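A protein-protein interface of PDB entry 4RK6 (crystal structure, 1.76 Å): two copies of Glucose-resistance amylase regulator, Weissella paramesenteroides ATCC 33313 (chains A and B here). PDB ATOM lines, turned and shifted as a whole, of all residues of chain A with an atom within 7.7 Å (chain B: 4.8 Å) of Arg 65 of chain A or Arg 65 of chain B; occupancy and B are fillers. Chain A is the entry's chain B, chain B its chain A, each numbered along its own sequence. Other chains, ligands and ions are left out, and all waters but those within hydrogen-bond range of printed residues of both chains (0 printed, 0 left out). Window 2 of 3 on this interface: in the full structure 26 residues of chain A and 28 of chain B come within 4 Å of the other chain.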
ATOM      1  N   ARG A  11      30.831  -5.356 -12.551  1.00  0.00           N
ATOM      2  CA  ARG A  11      29.803  -6.295 -13.086  1.00  0.00           C
ATOM      3  C   ARG A  11      29.150  -7.066 -11.931  1.00  0.00           C
ATOM      4  O   ARG A  11      29.497  -8.214 -11.642  1.00  0.00           O
ATOM      5  CB  ARG A  11      30.421  -7.265 -14.105  1.00  0.00           C
ATOM      6  CG  ARG A  11      31.374  -6.629 -15.108  1.00  0.00           C
ATOM      7  CD  ARG A  11      30.659  -5.762 -16.130  1.00  0.00           C
ATOM      8  NE  ARG A  11      30.443  -6.471 -17.390  1.00  0.00           N
ATOM      9  CZ  ARG A  11      30.028  -5.898 -18.518  1.00  0.00           C
ATOM     10  NH1 ARG A  11      29.767  -4.594 -18.567  1.00  0.00           N
ATOM     11  NH2 ARG A  11      29.869  -6.636 -19.612  1.00  0.00           N
ATOM     12  N   VAL A  12      28.193  -6.422 -11.271  1.00  0.00           N
ATOM     13  CA  VAL A  12      27.485  -7.030 -10.159  1.00  0.00           C
ATOM     14  C   VAL A  12      25.978  -6.912 -10.388  1.00  0.00           C
ATOM     15  O   VAL A  12      25.517  -5.904 -10.898  1.00  0.00           O
ATOM     16  CB  VAL A  12      27.847  -6.339  -8.835  1.00  0.00           C
ATOM     17  CG1 VAL A  12      27.224  -7.081  -7.664  1.00  0.00           C
ATOM     18  CG2 VAL A  12      29.358  -6.256  -8.682  1.00  0.00           C
ATOM     19  N   VAL A  13      25.249  -7.964 -10.024  1.00  0.00           N
ATOM     20  CA  VAL A  13      23.778  -7.947  -9.982  1.00  0.00           C
ATOM     21  C   VAL A  13      23.311  -8.306  -8.579  1.00  0.00           C
ATOM     22  O   VAL A  13      23.990  -9.041  -7.836  1.00  0.00           O
ATOM     23  CB  VAL A  13      23.117  -8.874 -11.018  1.00  0.00           C
ATOM     24  CG1 VAL A  13      23.530  -8.498 -12.428  1.00  0.00           C
ATOM     25  CG2 VAL A  13      23.417 -10.348 -10.740  1.00  0.00           C
ATOM     26  N   GLU A  42      29.156 -11.026 -10.750  1.00  0.00           N
ATOM     27  CA  GLU A  42      29.007 -11.575  -9.415  1.00  0.00           C
ATOM     28  C   GLU A  42      27.619 -11.271  -8.883  1.00  0.00           C
ATOM     29  O   GLU A  42      26.982 -10.336  -9.327  1.00  0.00           O
ATOM     30  CB  GLU A  42      30.092 -11.034  -8.483  1.00  0.00           C
ATOM     31  CG  GLU A  42      31.256 -12.004  -8.322  1.00  0.00           C
ATOM     32  CD  GLU A  42      30.804 -13.372  -7.825  1.00  0.00           C
ATOM     33  OE1 GLU A  42      31.256 -14.391  -8.393  1.00  0.00           O
ATOM     34  OE2 GLU A  42      29.977 -13.428  -6.884  1.00  0.00           O
ATOM     35  N   LEU A  44      25.038 -10.518  -5.619  1.00  0.00           N
ATOM     36  CA  LEU A  44      24.889 -10.054  -4.241  1.00  0.00           C
ATOM     37  C   LEU A  44      23.482 -10.385  -3.819  1.00  0.00           C
ATOM     38  O   LEU A  44      22.539 -10.066  -4.539  1.00  0.00           O
ATOM     39  CB  LEU A  44      25.056  -8.543  -4.135  1.00  0.00           C
ATOM     40  CG  LEU A  44      26.437  -7.918  -4.279  1.00  0.00           C
ATOM     41  CD1 LEU A  44      26.289  -6.407  -4.207  1.00  0.00           C
ATOM     42  CD2 LEU A  44      27.386  -8.427  -3.204  1.00  0.00           C
ATOM     43  N   GLN A  57      17.318   1.425   3.545  1.00  0.00           N
ATOM     44  CA  GLN A  57      18.752   1.164   3.797  1.00  0.00           C
ATOM     45  C   GLN A  57      19.306   0.192   2.765  1.00  0.00           C
ATOM     46  O   GLN A  57      20.362   0.430   2.181  1.00  0.00           O
ATOM     47  CB  GLN A  57      19.007   0.583   5.203  1.00  0.00           C
ATOM     48  CG  GLN A  57      18.455   1.379   6.377  1.00  0.00           C
ATOM     49  CD  GLN A  57      18.524   2.882   6.170  1.00  0.00           C
ATOM     50  OE1 GLN A  57      19.544   3.415   5.730  1.00  0.00           O
ATOM     51  NE2 GLN A  57      17.433   3.575   6.487  1.00  0.00           N
ATOM     52  N   VAL A  58      18.563  -0.889   2.545  1.00  0.00           N
ATOM     53  CA  VAL A  58      18.887  -1.902   1.551  1.00  0.00           C
ATOM     54  C   VAL A  58      19.043  -1.291   0.174  1.00  0.00           C
ATOM     55  O   VAL A  58      20.032  -1.547  -0.513  1.00  0.00           O
ATOM     56  CB  VAL A  58      17.789  -2.990   1.487  1.00  0.00           C
ATOM     57  CG1 VAL A  58      17.929  -3.869   0.248  1.00  0.00           C
ATOM     58  CG2 VAL A  58      17.823  -3.846   2.745  1.00  0.00           C
ATOM     59  N   PHE A  59      18.065  -0.492  -0.238  1.00  0.00           N
ATOM     60  CA  PHE A  59      18.148   0.147  -1.541  1.00  0.00           C
ATOM     61  C   PHE A  59      19.441   0.974  -1.693  1.00  0.00           C
ATOM     62  O   PHE A  59      20.107   0.908  -2.727  1.00  0.00           O
ATOM     63  CB  PHE A  59      16.896   0.998  -1.824  1.00  0.00           C
ATOM     64  CG  PHE A  59      17.131   2.061  -2.842  1.00  0.00           C
ATOM     65  CD1 PHE A  59      17.127   1.763  -4.193  1.00  0.00           C
ATOM     66  CD2 PHE A  59      17.398   3.365  -2.450  1.00  0.00           C
ATOM     67  CE1 PHE A  59      17.372   2.750  -5.132  1.00  0.00           C
ATOM     68  CE2 PHE A  59      17.656   4.347  -3.386  1.00  0.00           C
ATOM     69  CZ  PHE A  59      17.645   4.038  -4.732  1.00  0.00           C
ATOM     70  N   GLN A  60      19.810   1.750  -0.676  1.00  0.00           N
ATOM     71  CA  GLN A  60      21.087   2.476  -0.711  1.00  0.00           C
ATOM     72  C   GLN A  60      22.298   1.531  -0.856  1.00  0.00           C
ATOM     73  O   GLN A  60      23.293   1.919  -1.459  1.00  0.00           O
ATOM     74  CB  GLN A  60      21.244   3.362   0.524  1.00  0.00           C
ATOM     75  CG  GLN A  60      20.291   4.550   0.531  1.00  0.00           C
ATOM     76  CD  GLN A  60      20.263   5.301   1.853  1.00  0.00           C
ATOM     77  OE1 GLN A  60      20.022   6.507   1.883  1.00  0.00           O
ATOM     78  NE2 GLN A  60      20.499   4.591   2.953  1.00  0.00           N
ATOM     79  N   THR A  61      22.192   0.309  -0.318  1.00  0.00           N
ATOM     80  CA  THR A  61      23.201  -0.767  -0.507  1.00  0.00           C
ATOM     81  C   THR A  61      23.189  -1.349  -1.957  1.00  0.00           C
ATOM     82  O   THR A  61      24.222  -1.723  -2.469  1.00  0.00           O
ATOM     83  CB  THR A  61      23.044  -1.874   0.576  1.00  0.00           C
ATOM     84  OG1 THR A  61      23.663  -1.429   1.790  1.00  0.00           O
ATOM     85  CG2 THR A  61      23.680  -3.199   0.164  1.00  0.00           C
ATOM     86  N   LEU A  62      22.038  -1.406  -2.628  1.00  0.00           N
ATOM     87  CA  LEU A  62      22.003  -1.798  -4.050  1.00  0.00           C
ATOM     88  C   LEU A  62      22.534  -0.706  -4.957  1.00  0.00           C
ATOM     89  O   LEU A  62      23.320  -0.982  -5.862  1.00  0.00           O
ATOM     90  CB  LEU A  62      20.589  -2.165  -4.483  1.00  0.00           C
ATOM     91  CG  LEU A  62      20.012  -3.400  -3.791  1.00  0.00           C
ATOM     92  CD1 LEU A  62      18.492  -3.453  -3.921  1.00  0.00           C
ATOM     93  CD2 LEU A  62      20.666  -4.681  -4.293  1.00  0.00           C
ATOM     94  N   LEU A  63      22.099   0.534  -4.723  1.00  0.00           N
ATOM     95  CA  LEU A  63      22.635   1.681  -5.457  1.00  0.00           C
ATOM     96  C   LEU A  63      24.166   1.806  -5.268  1.00  0.00           C
ATOM     97  O   LEU A  63      24.902   1.967  -6.248  1.00  0.00           O
ATOM     98  CB  LEU A  63      21.923   2.954  -4.994  1.00  0.00           C
ATOM     99  CG  LEU A  63      22.153   4.292  -5.700  1.00  0.00           C
ATOM    100  CD1 LEU A  63      21.242   5.324  -5.055  1.00  0.00           C
ATOM    101  CD2 LEU A  63      23.598   4.778  -5.652  1.00  0.00           C
ATOM    102  N   SER A  64      24.631   1.704  -4.016  1.00  0.00           N
ATOM    103  CA  SER A  64      26.045   1.954  -3.665  1.00  0.00           C
ATOM    104  C   SER A  64      27.019   0.814  -3.991  1.00  0.00           C
ATOM    105  O   SER A  64      28.229   1.016  -3.962  1.00  0.00           O
ATOM    106  CB  SER A  64      26.187   2.320  -2.185  1.00  0.00           C
ATOM    107  OG  SER A  64      25.846   1.225  -1.351  1.00  0.00           O
ATOM    108  N   ARG A  65      26.513  -0.379  -4.293  1.00  0.00           N
ATOM    109  CA  ARG A  65      27.355  -1.398  -4.933  1.00  0.00           C
ATOM    110  C   ARG A  65      27.178  -1.327  -6.463  1.00  0.00           C
ATOM    111  O   ARG A  65      27.566  -2.248  -7.188  1.00  0.00           O
ATOM    112  CB  ARG A  65      27.057  -2.812  -4.386  1.00  0.00           C
ATOM    113  CG  ARG A  65      26.834  -2.919  -2.870  1.00  0.00           C
ATOM    114  CD  ARG A  65      27.900  -2.251  -1.990  1.00  0.00           C
ATOM    115  NE  ARG A  65      27.329  -1.467  -0.891  1.00  0.00           N
ATOM    116  CZ  ARG A  65      28.035  -0.776   0.006  1.00  0.00           C
ATOM    117  NH1 ARG A  65      29.366  -0.765  -0.023  1.00  0.00           N
ATOM    118  NH2 ARG A  65      27.399  -0.090   0.950  1.00  0.00           N
ATOM    119  N   GLN A  66      26.586  -0.231  -6.944  1.00  0.00           N
ATOM    120  CA  GLN A  66      26.451   0.044  -8.370  1.00  0.00           C
ATOM    121  C   GLN A  66      26.092  -1.219  -9.148  1.00  0.00           C
ATOM    122  O   GLN A  66      26.756  -1.571 -10.124  1.00  0.00           O
ATOM    123  CB  GLN A  66      27.739   0.674  -8.917  1.00  0.00           C
ATOM    124  N   VAL A  67      25.035  -1.895  -8.701  1.00  0.00           N
ATOM    125  CA  VAL A  67      24.542  -3.098  -9.376  1.00  0.00           C
ATOM    126  C   VAL A  67      23.979  -2.722 -10.748  1.00  0.00           C
ATOM    127  O   VAL A  67      23.474  -1.613 -10.932  1.00  0.00           O
ATOM    128  CB  VAL A  67      23.485  -3.865  -8.544  1.00  0.00           C
ATOM    129  CG1 VAL A  67      24.059  -4.277  -7.196  1.00  0.00           C
ATOM    130  CG2 VAL A  67      22.212  -3.046  -8.357  1.00  0.00           C
ATOM    131  N   GLY A  68      24.098  -3.632 -11.708  1.00  0.00           N
ATOM    132  CA  GLY A  68      23.592  -3.418 -13.060  1.00  0.00           C
ATOM    133  C   GLY A  68      22.137  -3.820 -13.198  1.00  0.00           C
ATOM    134  O   GLY A  68      21.422  -3.333 -14.086  1.00  0.00           O
ATOM    135  N   ILE A  90      19.167   1.173 -13.623  1.00  0.00           N
ATOM    136  CA  ILE A  90      19.378  -0.208 -13.200  1.00  0.00           C
ATOM    137  C   ILE A  90      18.203  -1.026 -13.709  1.00  0.00           C
ATOM    138  O   ILE A  90      17.035  -0.616 -13.566  1.00  0.00           O
ATOM    139  CB  ILE A  90      19.491  -0.286 -11.668  1.00  0.00           C
ATOM    140  CG1 ILE A  90      20.742   0.480 -11.212  1.00  0.00           C
ATOM    141  CG2 ILE A  90      19.522  -1.732 -11.186  1.00  0.00           C
ATOM    142  CD1 ILE A  90      20.817   0.747  -9.736  1.00  0.00           C
ATOM    143  N   VAL B  12      29.094  -1.760   6.013  1.00  0.00           N
ATOM    144  CA  VAL B  12      28.601  -3.015   5.470  1.00  0.00           C
ATOM    145  C   VAL B  12      29.457  -4.171   5.986  1.00  0.00           C
ATOM    146  O   VAL B  12      30.650  -3.974   6.180  1.00  0.00           O
ATOM    147  CB  VAL B  12      28.644  -3.007   3.933  1.00  0.00           C
ATOM    148  CG1 VAL B  12      28.232  -4.361   3.373  1.00  0.00           C
ATOM    149  CG2 VAL B  12      27.749  -1.905   3.395  1.00  0.00           C
ATOM    150  N   LEU B  44      25.699  -7.974   3.269  1.00  0.00           N
ATOM    151  CA  LEU B  44      25.853  -8.504   1.894  1.00  0.00           C
ATOM    152  C   LEU B  44      26.046 -10.003   2.008  1.00  0.00           C
ATOM    153  O   LEU B  44      26.912 -10.454   2.767  1.00  0.00           O
ATOM    154  CB  LEU B  44      27.077  -7.912   1.214  1.00  0.00           C
ATOM    155  CG  LEU B  44      26.924  -6.677   0.331  1.00  0.00           C
ATOM    156  CD1 LEU B  44      26.017  -5.627   0.960  1.00  0.00           C
ATOM    157  CD2 LEU B  44      28.310  -6.119   0.032  1.00  0.00           C
ATOM    158  N   THR B  61      34.765  -8.819  -4.908  1.00  0.00           N
ATOM    159  CA  THR B  61      33.444  -8.252  -4.563  1.00  0.00           C
ATOM    160  C   THR B  61      33.383  -7.815  -3.086  1.00  0.00           C
ATOM    161  O   THR B  61      32.769  -6.812  -2.743  1.00  0.00           O
ATOM    162  CB  THR B  61      32.330  -9.296  -4.837  1.00  0.00           C
ATOM    163  OG1 THR B  61      32.233  -9.525  -6.248  1.00  0.00           O
ATOM    164  CG2 THR B  61      30.967  -8.850  -4.303  1.00  0.00           C
ATOM    165  N   LEU B  62      34.038  -8.570  -2.217  1.00  0.00           N
ATOM    166  CA  LEU B  62      34.114  -8.206  -0.795  1.00  0.00           C
ATOM    167  C   LEU B  62      34.933  -6.945  -0.518  1.00  0.00           C
ATOM    168  O   LEU B  62      34.403  -6.026   0.106  1.00  0.00           O
ATOM    169  CB  LEU B  62      34.555  -9.403   0.052  1.00  0.00           C
ATOM    170  CG  LEU B  62      33.513 -10.540   0.075  1.00  0.00           C
ATOM    171  CD1 LEU B  62      34.078 -11.866   0.589  1.00  0.00           C
ATOM    172  CD2 LEU B  62      32.269 -10.174   0.864  1.00  0.00           C
ATOM    173  N   LEU B  63      36.179  -6.839  -0.987  1.00  0.00           N
ATOM    174  CA  LEU B  63      36.930  -5.592  -0.720  1.00  0.00           C
ATOM    175  C   LEU B  63      36.463  -4.380  -1.538  1.00  0.00           C
ATOM    176  O   LEU B  63      36.574  -3.243  -1.055  1.00  0.00           O
ATOM    177  CB  LEU B  63      38.454  -5.765  -0.784  1.00  0.00           C
ATOM    178  CG  LEU B  63      39.192  -5.880  -2.107  1.00  0.00           C
ATOM    179  CD1 LEU B  63      40.679  -5.616  -1.915  1.00  0.00           C
ATOM    180  CD2 LEU B  63      38.979  -7.247  -2.716  1.00  0.00           C
ATOM    181  N   SER B  64      35.905  -4.605  -2.731  1.00  0.00           N
ATOM    182  CA  SER B  64      35.375  -3.496  -3.548  1.00  0.00           C
ATOM    183  C   SER B  64      34.090  -2.891  -2.963  1.00  0.00           C
ATOM    184  O   SER B  64      33.781  -1.723  -3.209  1.00  0.00           O
ATOM    185  CB  SER B  64      35.151  -3.922  -5.008  1.00  0.00           C
ATOM    186  OG  SER B  64      34.149  -4.916  -5.117  1.00  0.00           O
ATOM    187  N   ARG B  65      33.358  -3.681  -2.176  1.00  0.00           N
ATOM    188  CA  ARG B  65      32.183  -3.192  -1.444  1.00  0.00           C
ATOM    189  C   ARG B  65      32.579  -2.678  -0.051  1.00  0.00           C
ATOM    190  O   ARG B  65      31.715  -2.305   0.747  1.00  0.00           O
ATOM    191  CB  ARG B  65      31.099  -4.283  -1.363  1.00  0.00           C
ATOM    192  CG  ARG B  65      30.214  -4.383  -2.607  1.00  0.00           C
ATOM    193  CD  ARG B  65      30.943  -4.717  -3.906  1.00  0.00           C
ATOM    194  NE  ARG B  65      30.344  -4.040  -5.060  1.00  0.00           N
ATOM    195  CZ  ARG B  65      30.790  -4.140  -6.313  1.00  0.00           C
ATOM    196  NH1 ARG B  65      31.854  -4.880  -6.608  1.00  0.00           N
ATOM    197  NH2 ARG B  65      30.165  -3.481  -7.283  1.00  0.00           N
ATOM    198  N   GLN B  66      33.885  -2.663   0.229  1.00  0.00           N
ATOM    199  CA  GLN B  66      34.443  -2.017   1.415  1.00  0.00           C
ATOM    200  C   GLN B  66      33.827  -2.554   2.705  1.00  0.00           C
ATOM    201  O   GLN B  66      33.492  -1.790   3.626  1.00  0.00           O
ATOM    202  CB  GLN B  66      34.264  -0.492   1.337  1.00  0.00           C
ATOM    203  CG  GLN B  66      34.812   0.133   0.061  1.00  0.00           C
ATOM    204  CD  GLN B  66      34.479   1.606  -0.051  1.00  0.00           C
ATOM    205  OE1 GLN B  66      33.887   2.046  -1.037  1.00  0.00           O
ATOM    206  NE2 GLN B  66      34.846   2.378   0.966  1.00  0.00           N
ATOM    207  N   VAL B  67      33.702  -3.868   2.785  1.00  0.00           N
ATOM    208  CA  VAL B  67      33.103  -4.468   3.975  1.00  0.00           C
ATOM    209  C   VAL B  67      34.030  -4.266   5.174  1.00  0.00           C
ATOM    210  O   VAL B  67      35.260  -4.225   5.030  1.00  0.00           O
ATOM    211  CB  VAL B  67      32.743  -5.953   3.773  1.00  0.00           C
ATOM    212  CG1 VAL B  67      31.748  -6.111   2.626  1.00  0.00           C
ATOM    213  CG2 VAL B  67      33.989  -6.795   3.530  1.00  0.00           C
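The guanidinium group (NH2) of Arg 65 of chain B lies within hydrogen-bond range of the backbone carbonyl oxygen (O) of Arg 65 of chain A (2.9 Å).
Among the printed residues, pairs that only touch across the chains: Val 12 of chain A with Arg 65 of chain B (3.2 Å), Glu 42 of chain A with Thr 61 of chain B (3.4 Å), Leu 44 of chain A with Leu 44 of chain B (3.97 Å), Leu 44 of chain A with Thr 61 of chain B (3.8 Å), Thr 61 of chain A with Leu 44 of chain B (3.5 Å) and Arg 65 of chain A with Val 12 of chain B (3.1 Å).
The backbone carbonyl oxygen of Glu 42 of chain A sits at hydrogen-bond distance from the backbone NH of Val 13 of chain A (3.0 Å).
The backbone NH of Leu 44 of chain A is in hydrogen-bond range of the backbone carbonyl oxygen of Val 13 of chain A.
The backbone carbonyl oxygen (O) of Arg 11 of chain A sits at hydrogen-bond distance from the backbone NH (N) of Glu 42 of chain A, at 3.0 Å.
O of Val 12 of chain A is in hydrogen-bond range of N of Gly 68 of chain A, 2.8 Å away.
O of Thr 61 of chain B lies within hydrogen-bond range of OG of Ser 64 of chain B.
NH2 of Arg 65 of chain A lies within hydrogen-bond range of OG of Ser 64 of chain A (3.1 Å).
Val 12 of chain A touches Arg 65 of chain B, and with the chains exchanged Arg 65 of chain A touches Val 12 of chain B.
Leu 44 of chain A touches its own counterpart, Leu 44 of chain B.
Leu 44 of chain A touches Thr 61 of chain B, and with the chains exchanged Thr 61 of chain A touches Leu 44 of chain B.
Arg 65 of chain B touches its own counterpart, Arg 65 of chain A.
Positions printed for both chains: 12, 44, 61, 62, 63, 64, 65, 66 and 67.
Printed residues of chain B within 4 Å of Glu 42 of chain A: Thr 61 (3.4 Å).
Printed residues of chain B within 4 Å of Leu 44 of chain A: Leu 44 (3.97 Å) and Thr 61 (3.8 Å).
Printed residues of chain B within 4 Å of Arg 65 of chain A: Val 12 (3.1 Å) and Arg 65 (2.9 Å).
Ile 90 of chain A touches none of the printed residues of chain B.
Leu 62 of chain B touches none of the printed residues of chain A.
Ser 64 of chain B touches none of the printed residues of chain A.
Arg 65 of chain B touches just these residues of chain A: Val 12 and Arg 65.
The nearest printed residue of chain B that does not touch Leu 44 of chain A is Arg 65 of chain B (4.7 Å).
Hydrophobic or aromatic side chains of chain A within 4 Å of the printed part of chain B: Val 12 and Leu 44.
Along chain A the printed residues that touch a printed residue of chain B span positions 12 to 65.
Among the printed residues, 7 pairs touch across the chains.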
